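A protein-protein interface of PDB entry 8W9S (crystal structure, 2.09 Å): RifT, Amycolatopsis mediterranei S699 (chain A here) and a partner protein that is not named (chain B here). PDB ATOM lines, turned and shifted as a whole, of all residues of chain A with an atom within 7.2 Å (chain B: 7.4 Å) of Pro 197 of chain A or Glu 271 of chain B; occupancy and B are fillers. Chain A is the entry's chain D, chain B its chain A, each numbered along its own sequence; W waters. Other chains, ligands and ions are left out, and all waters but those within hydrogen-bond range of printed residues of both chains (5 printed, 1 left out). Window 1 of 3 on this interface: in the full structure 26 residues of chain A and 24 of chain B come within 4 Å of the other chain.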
ATOM      1  N   GLU A  82      -1.218   4.274 -35.246  1.00  0.00           N
ATOM      2  CA  GLU A  82      -2.388   4.993 -35.740  1.00  0.00           C
ATOM      3  C   GLU A  82      -2.802   6.082 -34.755  1.00  0.00           C
ATOM      4  O   GLU A  82      -3.229   7.168 -35.163  1.00  0.00           O
ATOM      5  CB  GLU A  82      -3.544   4.014 -35.981  1.00  0.00           C
ATOM      6  CG  GLU A  82      -4.839   4.665 -36.493  1.00  0.00           C
ATOM      7  CD  GLU A  82      -4.598   5.684 -37.611  1.00  0.00           C
ATOM      8  OE1 GLU A  82      -3.883   5.345 -38.594  1.00  0.00           O
ATOM      9  OE2 GLU A  82      -5.134   6.816 -37.512  1.00  0.00           O
ATOM     10  N   ALA A  83      -2.672   5.803 -33.450  1.00  0.00           N
ATOM     11  CA  ALA A  83      -2.943   6.811 -32.429  1.00  0.00           C
ATOM     12  C   ALA A  83      -2.075   8.051 -32.615  1.00  0.00           C
ATOM     13  O   ALA A  83      -2.544   9.175 -32.415  1.00  0.00           O
ATOM     14  CB  ALA A  83      -2.716   6.220 -31.034  1.00  0.00           C
ATOM     15  N   PHE A  84      -0.795   7.872 -32.958  1.00  0.00           N
ATOM     16  CA  PHE A  84       0.068   9.037 -33.141  1.00  0.00           C
ATOM     17  C   PHE A  84      -0.349   9.859 -34.362  1.00  0.00           C
ATOM     18  O   PHE A  84      -0.251  11.093 -34.346  1.00  0.00           O
ATOM     19  CB  PHE A  84       1.538   8.616 -33.268  1.00  0.00           C
ATOM     20  CG  PHE A  84       2.514   9.785 -33.232  1.00  0.00           C
ATOM     21  CD1 PHE A  84       2.351  10.816 -32.313  1.00  0.00           C
ATOM     22  CD2 PHE A  84       3.575   9.855 -34.123  1.00  0.00           C
ATOM     23  CE1 PHE A  84       3.234  11.897 -32.272  1.00  0.00           C
ATOM     24  CE2 PHE A  84       4.462  10.932 -34.090  1.00  0.00           C
ATOM     25  CZ  PHE A  84       4.291  11.952 -33.163  1.00  0.00           C
ATOM     26  N   VAL A  87      -3.077  12.072 -33.198  1.00  0.00           N
ATOM     27  CA  VAL A  87      -2.629  13.194 -32.381  1.00  0.00           C
ATOM     28  C   VAL A  87      -1.992  14.277 -33.250  1.00  0.00           C
ATOM     29  O   VAL A  87      -2.269  15.470 -33.082  1.00  0.00           O
ATOM     30  CB  VAL A  87      -1.672  12.701 -31.279  1.00  0.00           C
ATOM     31  CG1 VAL A  87      -0.997  13.888 -30.592  1.00  0.00           C
ATOM     32  CG2 VAL A  87      -2.449  11.856 -30.254  1.00  0.00           C
ATOM     33  N   LEU A 179       8.197   1.793 -23.753  1.00  0.00           N
ATOM     34  CA  LEU A 179       7.106   2.472 -24.448  1.00  0.00           C
ATOM     35  C   LEU A 179       6.896   3.863 -23.867  1.00  0.00           C
ATOM     36  O   LEU A 179       6.603   3.985 -22.669  1.00  0.00           O
ATOM     37  CB  LEU A 179       5.816   1.679 -24.360  1.00  0.00           C
ATOM     38  CG  LEU A 179       5.897   0.298 -25.007  1.00  0.00           C
ATOM     39  CD1 LEU A 179       4.685  -0.531 -24.657  1.00  0.00           C
ATOM     40  CD2 LEU A 179       6.063   0.431 -26.518  1.00  0.00           C
ATOM     41  N   PRO A 180       6.982   4.914 -24.674  1.00  0.00           N
ATOM     42  CA  PRO A 180       6.867   6.277 -24.156  1.00  0.00           C
ATOM     43  C   PRO A 180       5.427   6.753 -24.039  1.00  0.00           C
ATOM     44  O   PRO A 180       4.505   6.241 -24.679  1.00  0.00           O
ATOM     45  CB  PRO A 180       7.609   7.103 -25.210  1.00  0.00           C
ATOM     46  CG  PRO A 180       7.348   6.359 -26.491  1.00  0.00           C
ATOM     47  CD  PRO A 180       7.267   4.889 -26.122  1.00  0.00           C
ATOM     48  N   VAL A 182       3.822  10.720 -24.204  1.00  0.00           N
ATOM     49  CA  VAL A 182       4.214  12.091 -24.495  1.00  0.00           C
ATOM     50  C   VAL A 182       2.975  12.963 -24.380  1.00  0.00           C
ATOM     51  O   VAL A 182       1.858  12.518 -24.676  1.00  0.00           O
ATOM     52  CB  VAL A 182       4.896  12.201 -25.882  1.00  0.00           C
ATOM     53  CG1 VAL A 182       3.893  11.993 -27.023  1.00  0.00           C
ATOM     54  CG2 VAL A 182       5.611  13.500 -26.035  1.00  0.00           C
ATOM     55  N   VAL A 191      -2.959  17.348 -24.914  1.00  0.00           N
ATOM     56  CA  VAL A 191      -3.347  15.995 -25.296  1.00  0.00           C
ATOM     57  C   VAL A 191      -2.157  15.079 -25.070  1.00  0.00           C
ATOM     58  O   VAL A 191      -1.005  15.477 -25.287  1.00  0.00           O
ATOM     59  CB  VAL A 191      -3.805  15.930 -26.764  1.00  0.00           C
ATOM     60  CG1 VAL A 191      -2.711  16.466 -27.671  1.00  0.00           C
ATOM     61  CG2 VAL A 191      -4.186  14.493 -27.144  1.00  0.00           C
ATOM     62  N   GLN A 192      -2.433  13.854 -24.632  1.00  0.00           N
ATOM     63  CA  GLN A 192      -1.405  12.874 -24.318  1.00  0.00           C
ATOM     64  C   GLN A 192      -1.463  11.719 -25.305  1.00  0.00           C
ATOM     65  O   GLN A 192      -2.542  11.171 -25.573  1.00  0.00           O
ATOM     66  CB  GLN A 192      -1.570  12.339 -22.886  1.00  0.00           C
ATOM     67  CG  GLN A 192      -0.676  11.154 -22.603  1.00  0.00           C
ATOM     68  CD  GLN A 192      -0.905  10.545 -21.214  1.00  0.00           C
ATOM     69  OE1 GLN A 192      -1.919   9.867 -20.960  1.00  0.00           O
ATOM     70  NE2 GLN A 192       0.041  10.776 -20.320  1.00  0.00           N
ATOM     71  N   TYR A 193      -0.303  11.333 -25.819  1.00  0.00           N
ATOM     72  CA  TYR A 193      -0.132  10.101 -26.568  1.00  0.00           C
ATOM     73  C   TYR A 193       0.677   9.134 -25.713  1.00  0.00           C
ATOM     74  O   TYR A 193       1.830   9.419 -25.373  1.00  0.00           O
ATOM     75  CB  TYR A 193       0.564  10.372 -27.900  1.00  0.00           C
ATOM     76  CG  TYR A 193       0.970   9.133 -28.634  1.00  0.00           C
ATOM     77  CD1 TYR A 193       0.100   8.061 -28.755  1.00  0.00           C
ATOM     78  CD2 TYR A 193       2.229   9.028 -29.222  1.00  0.00           C
ATOM     79  CE1 TYR A 193       0.479   6.898 -29.433  1.00  0.00           C
ATOM     80  CE2 TYR A 193       2.615   7.868 -29.909  1.00  0.00           C
ATOM     81  CZ  TYR A 193       1.730   6.813 -30.014  1.00  0.00           C
ATOM     82  OH  TYR A 193       2.092   5.661 -30.679  1.00  0.00           O
ATOM     83  N   ASP A 194       0.062   8.009 -25.350  1.00  0.00           N
ATOM     84  CA  ASP A 194       0.665   6.974 -24.512  1.00  0.00           C
ATOM     85  C   ASP A 194       0.757   5.725 -25.375  1.00  0.00           C
ATOM     86  O   ASP A 194      -0.273   5.163 -25.773  1.00  0.00           O
ATOM     87  CB  ASP A 194      -0.189   6.742 -23.255  1.00  0.00           C
ATOM     88  CG  ASP A 194       0.367   5.667 -22.319  1.00  0.00           C
ATOM     89  OD1 ASP A 194       1.414   5.043 -22.602  1.00  0.00           O
ATOM     90  OD2 ASP A 194      -0.287   5.444 -21.276  1.00  0.00           O
ATOM     91  N   ALA A 195       1.983   5.291 -25.668  1.00  0.00           N
ATOM     92  CA  ALA A 195       2.160   4.102 -26.485  1.00  0.00           C
ATOM     93  C   ALA A 195       1.938   2.814 -25.713  1.00  0.00           C
ATOM     94  O   ALA A 195       1.869   1.749 -26.338  1.00  0.00           O
ATOM     95  CB  ALA A 195       3.551   4.064 -27.093  1.00  0.00           C
ATOM     96  N   GLY A 196       1.854   2.873 -24.387  1.00  0.00           N
ATOM     97  CA  GLY A 196       1.689   1.672 -23.595  1.00  0.00           C
ATOM     98  C   GLY A 196       0.694   1.857 -22.467  1.00  0.00           C
ATOM     99  O   GLY A 196       1.039   1.780 -21.287  1.00  0.00           O
ATOM    100  N   PRO A 197      -0.562   2.131 -22.806  1.00  0.00           N
ATOM    101  CA  PRO A 197      -1.566   2.335 -21.755  1.00  0.00           C
ATOM    102  C   PRO A 197      -1.916   1.021 -21.073  1.00  0.00           C
ATOM    103  O   PRO A 197      -1.645  -0.071 -21.584  1.00  0.00           O
ATOM    104  CB  PRO A 197      -2.766   2.904 -22.519  1.00  0.00           C
ATOM    105  CG  PRO A 197      -2.666   2.238 -23.887  1.00  0.00           C
ATOM    106  CD  PRO A 197      -1.167   2.086 -24.157  1.00  0.00           C
ATOM    107  N   GLN A 198      -2.517   1.146 -19.887  1.00  0.00           N
ATOM    108  CA  GLN A 198      -3.050  -0.009 -19.165  1.00  0.00           C
ATOM    109  C   GLN A 198      -4.367  -0.460 -19.793  1.00  0.00           C
ATOM    110  O   GLN A 198      -5.348   0.297 -19.830  1.00  0.00           O
ATOM    111  CB  GLN A 198      -3.266   0.315 -17.687  1.00  0.00           C
ATOM    112  CG  GLN A 198      -4.115  -0.752 -16.957  1.00  0.00           C
ATOM    113  CD  GLN A 198      -4.347  -0.424 -15.478  1.00  0.00           C
ATOM    114  OE1 GLN A 198      -3.406  -0.407 -14.692  1.00  0.00           O
ATOM    115  NE2 GLN A 198      -5.604  -0.176 -15.102  1.00  0.00           N
ATOM    116  N   LEU A 199      -4.392  -1.702 -20.271  1.00  0.00           N
ATOM    117  CA  LEU A 199      -5.621  -2.278 -20.814  1.00  0.00           C
ATOM    118  C   LEU A 199      -6.492  -2.853 -19.704  1.00  0.00           C
ATOM    119  O   LEU A 199      -7.675  -2.514 -19.589  1.00  0.00           O
ATOM    120  CB  LEU A 199      -5.277  -3.366 -21.831  1.00  0.00           C
ATOM    121  CG  LEU A 199      -6.429  -4.101 -22.534  1.00  0.00           C
ATOM    122  CD1 LEU A 199      -7.397  -3.103 -23.152  1.00  0.00           C
ATOM    123  CD2 LEU A 199      -5.895  -5.078 -23.597  1.00  0.00           C
ATOM    124  N   LEU A 200      -5.918  -3.729 -18.880  1.00  0.00           N
ATOM    125  CA  LEU A 200      -6.613  -4.342 -17.754  1.00  0.00           C
ATOM    126  C   LEU A 200      -5.898  -4.023 -16.442  1.00  0.00           C
ATOM    127  O   LEU A 200      -4.661  -4.054 -16.361  1.00  0.00           O
ATOM    128  CB  LEU A 200      -6.724  -5.870 -17.924  1.00  0.00           C
ATOM    129  CG  LEU A 200      -7.352  -6.367 -19.233  1.00  0.00           C
ATOM    130  CD1 LEU A 200      -7.362  -7.907 -19.301  1.00  0.00           C
ATOM    131  CD2 LEU A 200      -8.746  -5.802 -19.411  1.00  0.00           C
ATOM    132  N   GLU A 206      -2.409  -5.472 -17.330  1.00  0.00           N
ATOM    133  CA  GLU A 206      -2.148  -5.911 -18.691  1.00  0.00           C
ATOM    134  C   GLU A 206      -1.963  -4.696 -19.574  1.00  0.00           C
ATOM    135  O   GLU A 206      -2.717  -3.719 -19.484  1.00  0.00           O
ATOM    136  CB  GLU A 206      -3.276  -6.788 -19.229  1.00  0.00           C
ATOM    137  CG  GLU A 206      -3.213  -8.212 -18.718  1.00  0.00           C
ATOM    138  CD  GLU A 206      -2.026  -8.973 -19.285  1.00  0.00           C
ATOM    139  OE1 GLU A 206      -1.715  -8.796 -20.498  1.00  0.00           O
ATOM    140  OE2 GLU A 206      -1.428  -9.761 -18.518  1.00  0.00           O
ATOM    141  N   LEU A 207      -0.973  -4.767 -20.434  1.00  0.00           N
ATOM    142  CA  LEU A 207      -0.554  -3.588 -21.159  1.00  0.00           C
ATOM    143  C   LEU A 207      -1.383  -3.567 -22.439  1.00  0.00           C
ATOM    144  O   LEU A 207      -1.568  -4.606 -23.072  1.00  0.00           O
ATOM    145  CB  LEU A 207       0.948  -3.694 -21.434  1.00  0.00           C
ATOM    146  CG  LEU A 207       1.713  -2.425 -21.693  1.00  0.00           C
ATOM    147  CD1 LEU A 207       1.700  -1.725 -20.308  1.00  0.00           C
ATOM    148  CD2 LEU A 207       3.109  -2.710 -22.183  1.00  0.00           C
ATOM    149  N   GLY A 208      -1.949  -2.414 -22.782  1.00  0.00           N
ATOM    150  CA  GLY A 208      -2.733  -2.320 -24.004  1.00  0.00           C
ATOM    151  C   GLY A 208      -1.877  -1.908 -25.182  1.00  0.00           C
ATOM    152  O   GLY A 208      -0.756  -2.396 -25.316  1.00  0.00           O
ATOM    153  N   GLY A 209      -2.380  -1.037 -26.047  1.00  0.00           N
ATOM    154  CA  GLY A 209      -1.575  -0.457 -27.107  1.00  0.00           C
ATOM    155  C   GLY A 209      -1.728  -1.160 -28.447  1.00  0.00           C
ATOM    156  O   GLY A 209      -2.414  -2.177 -28.598  1.00  0.00           O
ATOM    157  N   GLU A 210      -1.060  -0.580 -29.440  1.00  0.00           N
ATOM    158  CA  GLU A 210      -1.032  -1.110 -30.797  1.00  0.00           C
ATOM    159  C   GLU A 210       0.153  -2.052 -30.967  1.00  0.00           C
ATOM    160  O   GLU A 210       1.092  -2.064 -30.172  1.00  0.00           O
ATOM    161  CB  GLU A 210      -0.938   0.026 -31.817  1.00  0.00           C
ATOM    162  CG  GLU A 210      -2.003   1.109 -31.681  1.00  0.00           C
ATOM    163  CD  GLU A 210      -1.847   2.219 -32.722  1.00  0.00           C
ATOM    164  OE1 GLU A 210      -1.736   3.405 -32.335  1.00  0.00           O
ATOM    165  OE2 GLU A 210      -1.845   1.903 -33.931  1.00  0.00           O
ATOM    166  N   TRP B 268     -11.451   4.339 -18.870  1.00  0.00           N
ATOM    167  CA  TRP B 268     -10.038   4.612 -18.616  1.00  0.00           C
ATOM    168  C   TRP B 268      -9.402   5.175 -19.886  1.00  0.00           C
ATOM    169  O   TRP B 268      -9.751   4.743 -20.992  1.00  0.00           O
ATOM    170  CB  TRP B 268      -9.274   3.342 -18.218  1.00  0.00           C
ATOM    171  CG  TRP B 268      -9.591   2.729 -16.896  1.00  0.00           C
ATOM    172  CD1 TRP B 268     -10.148   3.345 -15.810  1.00  0.00           C
ATOM    173  CD2 TRP B 268      -9.357   1.357 -16.510  1.00  0.00           C
ATOM    174  NE1 TRP B 268     -10.280   2.440 -14.777  1.00  0.00           N
ATOM    175  CE2 TRP B 268      -9.807   1.216 -15.183  1.00  0.00           C
ATOM    176  CE3 TRP B 268      -8.806   0.238 -17.164  1.00  0.00           C
ATOM    177  CZ2 TRP B 268      -9.718   0.000 -14.479  1.00  0.00           C
ATOM    178  CZ3 TRP B 268      -8.723  -0.968 -16.475  1.00  0.00           C
ATOM    179  CH2 TRP B 268      -9.179  -1.077 -15.137  1.00  0.00           C
ATOM    180  N   PRO B 269      -8.452   6.107 -19.767  1.00  0.00           N
ATOM    181  CA  PRO B 269      -7.759   6.614 -20.967  1.00  0.00           C
ATOM    182  C   PRO B 269      -6.878   5.539 -21.590  1.00  0.00           C
ATOM    183  O   PRO B 269      -6.265   4.731 -20.891  1.00  0.00           O
ATOM    184  CB  PRO B 269      -6.917   7.774 -20.422  1.00  0.00           C
ATOM    185  CG  PRO B 269      -6.618   7.337 -18.980  1.00  0.00           C
ATOM    186  CD  PRO B 269      -7.927   6.710 -18.523  1.00  0.00           C
ATOM    187  N   GLN B 270      -6.813   5.530 -22.916  1.00  0.00           N
ATOM    188  CA  GLN B 270      -5.931   4.583 -23.593  1.00  0.00           C
ATOM    189  C   GLN B 270      -4.822   5.333 -24.346  1.00  0.00           C
ATOM    190  O   GLN B 270      -4.096   6.128 -23.730  1.00  0.00           O
ATOM    191  CB  GLN B 270      -6.761   3.664 -24.494  1.00  0.00           C
ATOM    192  CG  GLN B 270      -7.643   2.665 -23.691  1.00  0.00           C
ATOM    193  CD  GLN B 270      -6.837   1.721 -22.820  1.00  0.00           C
ATOM    194  OE1 GLN B 270      -5.754   1.287 -23.211  1.00  0.00           O
ATOM    195  NE2 GLN B 270      -7.369   1.374 -21.642  1.00  0.00           N
ATOM    196  N   GLU B 271      -4.676   5.117 -25.664  1.00  0.00           N
ATOM    197  CA  GLU B 271      -3.520   5.681 -26.367  1.00  0.00           C
ATOM    198  C   GLU B 271      -3.631   7.184 -26.569  1.00  0.00           C
ATOM    199  O   GLU B 271      -2.604   7.871 -26.595  1.00  0.00           O
ATOM    200  CB  GLU B 271      -3.317   5.025 -27.731  1.00  0.00           C
ATOM    201  CG  GLU B 271      -2.929   3.570 -27.672  1.00  0.00           C
ATOM    202  CD  GLU B 271      -4.161   2.671 -27.647  1.00  0.00           C
ATOM    203  OE1 GLU B 271      -5.279   3.210 -27.493  1.00  0.00           O
ATOM    204  OE2 GLU B 271      -4.010   1.435 -27.767  1.00  0.00           O
ATOM    205  N   VAL B 272      -4.843   7.715 -26.729  1.00  0.00           N
ATOM    206  CA  VAL B 272      -5.045   9.127 -27.015  1.00  0.00           C
ATOM    207  C   VAL B 272      -5.921   9.710 -25.928  1.00  0.00           C
ATOM    208  O   VAL B 272      -7.068   9.278 -25.760  1.00  0.00           O
ATOM    209  CB  VAL B 272      -5.701   9.354 -28.386  1.00  0.00           C
ATOM    210  CG1 VAL B 272      -5.993  10.833 -28.571  1.00  0.00           C
ATOM    211  CG2 VAL B 272      -4.827   8.783 -29.506  1.00  0.00           C
ATOM    212  N   ARG B 273      -5.419  10.736 -25.240  1.00  0.00           N
ATOM    213  CA  ARG B 273      -6.144  11.319 -24.116  1.00  0.00           C
ATOM    214  C   ARG B 273      -6.028  12.837 -24.139  1.00  0.00           C
ATOM    215  O   ARG B 273      -4.924  13.385 -24.016  1.00  0.00           O
ATOM    216  CB  ARG B 273      -5.613  10.759 -22.790  1.00  0.00           C
ATOM    217  CG  ARG B 273      -6.280  11.341 -21.555  1.00  0.00           C
ATOM    218  CD  ARG B 273      -5.415  11.049 -20.306  1.00  0.00           C
ATOM    219  NE  ARG B 273      -5.941  11.693 -19.105  1.00  0.00           N
ATOM    220  CZ  ARG B 273      -5.398  11.577 -17.899  1.00  0.00           C
ATOM    221  NH1 ARG B 273      -4.309  10.836 -17.733  1.00  0.00           N
ATOM    222  NH2 ARG B 273      -5.946  12.207 -16.869  1.00  0.00           N
ATOM    223  N   TYR B 284     -10.198   8.472 -31.165  1.00  0.00           N
ATOM    224  CA  TYR B 284      -9.454   7.274 -31.535  1.00  0.00           C
ATOM    225  C   TYR B 284     -10.020   6.112 -30.744  1.00  0.00           C
ATOM    226  O   TYR B 284     -10.081   6.179 -29.511  1.00  0.00           O
ATOM    227  CB  TYR B 284      -7.953   7.414 -31.261  1.00  0.00           C
ATOM    228  CG  TYR B 284      -7.194   6.122 -31.453  1.00  0.00           C
ATOM    229  CD1 TYR B 284      -6.901   5.655 -32.727  1.00  0.00           C
ATOM    230  CD2 TYR B 284      -6.791   5.356 -30.372  1.00  0.00           C
ATOM    231  CE1 TYR B 284      -6.219   4.463 -32.916  1.00  0.00           C
ATOM    232  CE2 TYR B 284      -6.106   4.172 -30.547  1.00  0.00           C
ATOM    233  CZ  TYR B 284      -5.822   3.730 -31.828  1.00  0.00           C
ATOM    234  OH  TYR B 284      -5.141   2.549 -32.028  1.00  0.00           O
ATOM    235  N   GLY B 285     -10.420   5.052 -31.443  1.00  0.00           N
ATOM    236  CA  GLY B 285     -11.071   3.936 -30.783  1.00  0.00           C
ATOM    237  C   GLY B 285     -10.388   2.599 -30.978  1.00  0.00           C
ATOM    238  O   GLY B 285     -10.985   1.551 -30.717  1.00  0.00           O
ATOM    239  N   GLY B 286      -9.137   2.619 -31.428  1.00  0.00           N
ATOM    240  CA  GLY B 286      -8.421   1.404 -31.734  1.00  0.00           C
ATOM    241  C   GLY B 286      -8.846   0.760 -33.047  1.00  0.00           C
ATOM    242  O   GLY B 286      -9.564   1.344 -33.869  1.00  0.00           O
ATOM    243  N   PRO B 287      -8.393  -0.473 -33.261  1.00  0.00           N
ATOM    244  CA  PRO B 287      -8.786  -1.212 -34.467  1.00  0.00           C
ATOM    245  C   PRO B 287     -10.277  -1.527 -34.489  1.00  0.00           C
ATOM    246  O   PRO B 287     -10.873  -1.887 -33.472  1.00  0.00           O
ATOM    247  CB  PRO B 287      -7.955  -2.499 -34.378  1.00  0.00           C
ATOM    248  CG  PRO B 287      -6.844  -2.188 -33.384  1.00  0.00           C
ATOM    249  CD  PRO B 287      -7.467  -1.243 -32.412  1.00  0.00           C
HETATM  250  O   HOH W   1      -3.275   8.370 -19.147  1.00  0.00           O
HETATM  251  O   HOH W   2      -5.016   0.080 -25.644  1.00  0.00           O
HETATM  252  O   HOH W   3      -3.349   4.184 -19.100  1.00  0.00           O
HETATM  253  O   HOH W   4      -5.699   2.908 -18.885  1.00  0.00           O
HETATM  254  O   HOH W   5      -3.013   6.134 -21.136  1.00  0.00           O
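Hydrophobic or aromatic side chains of chain B that line the printed part of chain A: Trp 268, Val 272 and Tyr 284.
Of the 22 printed residues of chain A, 12 touch a printed residue of chain B.
Hydrophobic or aromatic side chains of chain A that line the printed part of chain B: Ala 83, Val 87, Val 191, Tyr 193 and Pro 197.
Among the printed residues, no Asp or Glu carboxylate lies within 4 Å of a Lys or Arg side-chain nitrogen of the other chain.
Among the printed residues, pairs that only touch across the chains: Glu 82 of chain A with Tyr 284 of chain B (3.8 Å), Ala 83 of chain A with Glu 271 of chain B (3.6 Å), Ala 83 of chain A with Val 272 of chain B (3.7 Å), Ala 83 of chain A with Tyr 284 of chain B (3.8 Å), Val 87 of chain A with Val 272 of chain B (3.96 Å), Val 191 of chain A with Arg 273 of chain B (3.3 Å), Gln 192 of chain A with Val 272 of chain B (3.5 Å), Tyr 193 of chain A with Glu 271 of chain B (3.3 Å), Asp 194 of chain A with Gln 270 of chain B (3.98 Å), Pro 197 of chain A with Gln 270 of chain B (3.3 Å), Pro 197 of chain A with Glu 271 of chain B (3.9 Å), Gln 198 of chain A with Trp 268 of chain B (3.5 Å), Leu 199 of chain A with Trp 268 of chain B (3.6 Å), Glu 210 of chain A with Glu 271 of chain B (3.9 Å) and Glu 210 of chain A with Tyr 284 of chain B (3.4 Å).
Water W2 lies within hydrogen-bond range of OE2 of Glu 271 of chain B (2.7 Å), OE1 of Gln 270 of chain B (2.8 Å) and N of Gly 209 of chain A (2.9 Å).
Water W1 lies within hydrogen-bond range of OE1 of Gln 192 of chain A (2.7 Å) and NH1 of Arg 273 of chain B (3.0 Å).
Water W4 lies within hydrogen-bond range of O of Pro 269 of chain B (2.8 Å) and O of Gln 198 of chain A (2.8 Å).
Water W5 bridges the backbone carbonyl oxygen of Gln 270 of chain B (2.8 Å) and the side-chain carboxylate of Asp 194 of chain A (2.8 Å).
Water W3 bridges the backbone NH (N) of Gln 198 of chain A (3.2 Å) and the backbone carbonyl oxygen (O) of Pro 269 of chain B (3.5 Å).
Of chain B, only Gln 270 (3.3 Å) and Glu 271 (3.9 Å) come within 4 Å of Pro 197 of chain A.
No residue of chain B comes within 4 Å of Gly 196 of chain A.
Printed residues of chain B within 4 Å of Gly 209 of chain A: Glu 271.
Printed residues of chain B within 4 Å of Glu 210 of chain A: Glu 271 (3.9 Å) and Tyr 284 (3.4 Å).
Of the printed residues of chain B, Val 191 of chain A touches Arg 273 (3.3 Å).
Of the printed residues of chain B, Gln 192 of chain A touches Glu 271 (3.5 Å), Val 272 (3.5 Å) and Arg 273 (2.6 Å).
Printed residues of chain A within 4 Å of Gln 270 of chain B: Asp 194 (3.98 Å), Pro 197 (3.3 Å) and Gln 198 (2.9 Å).
Val 182 of chain A touches none of the printed residues of chain B.
The nearest printed residue of chain A that does not touch Gln 270 of chain B is Leu 199 of chain A (4.1 Å).
O of Gln 198 of chain A is in hydrogen-bond range of NE2 of Gln 270 of chain B.
N of Asp 194 of chain A is in hydrogen-bond range of O of Glu 271 of chain B (2.9 Å).
OE2 of Glu 271 of chain B sits close to N of Gly 209 of chain A (3.4 Å).
The backbone carbonyl oxygen (O) of Arg 273 of chain B is in hydrogen-bond range of the backbone NH (N) of Gln 192 of chain A (2.6 Å).
The backbone carbonyl oxygen (O) of Glu 271 of chain B sits close to the backbone carbonyl oxygen (O) of Gln 192 of chain A, 3.5 Å away.
The backbone NH (N) of Glu 82 of chain A sits at hydrogen-bond distance from the side-chain carboxylate (OE2) of Glu 210 of chain A.
The backbone NH of Ala 83 of chain A is in hydrogen-bond range of the side-chain carboxylate of Glu 210 of chain A (2.8 Å).
The backbone NH of Val 182 of chain A lies within hydrogen-bond range of the backbone carbonyl oxygen of Tyr 193 of chain A (2.7 Å).
The side-chain carboxylate (OD1) of Asp 194 of chain A sits at hydrogen-bond distance from the backbone NH (N) of Gly 196 of chain A (2.8 Å).
N of Gly 208 of chain A is in hydrogen-bond range of O of Pro 197 of chain A.
The backbone NH (N) of Leu 199 of chain A is in hydrogen-bond range of the backbone carbonyl oxygen (O) of Glu 206 of chain A (2.7 Å).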
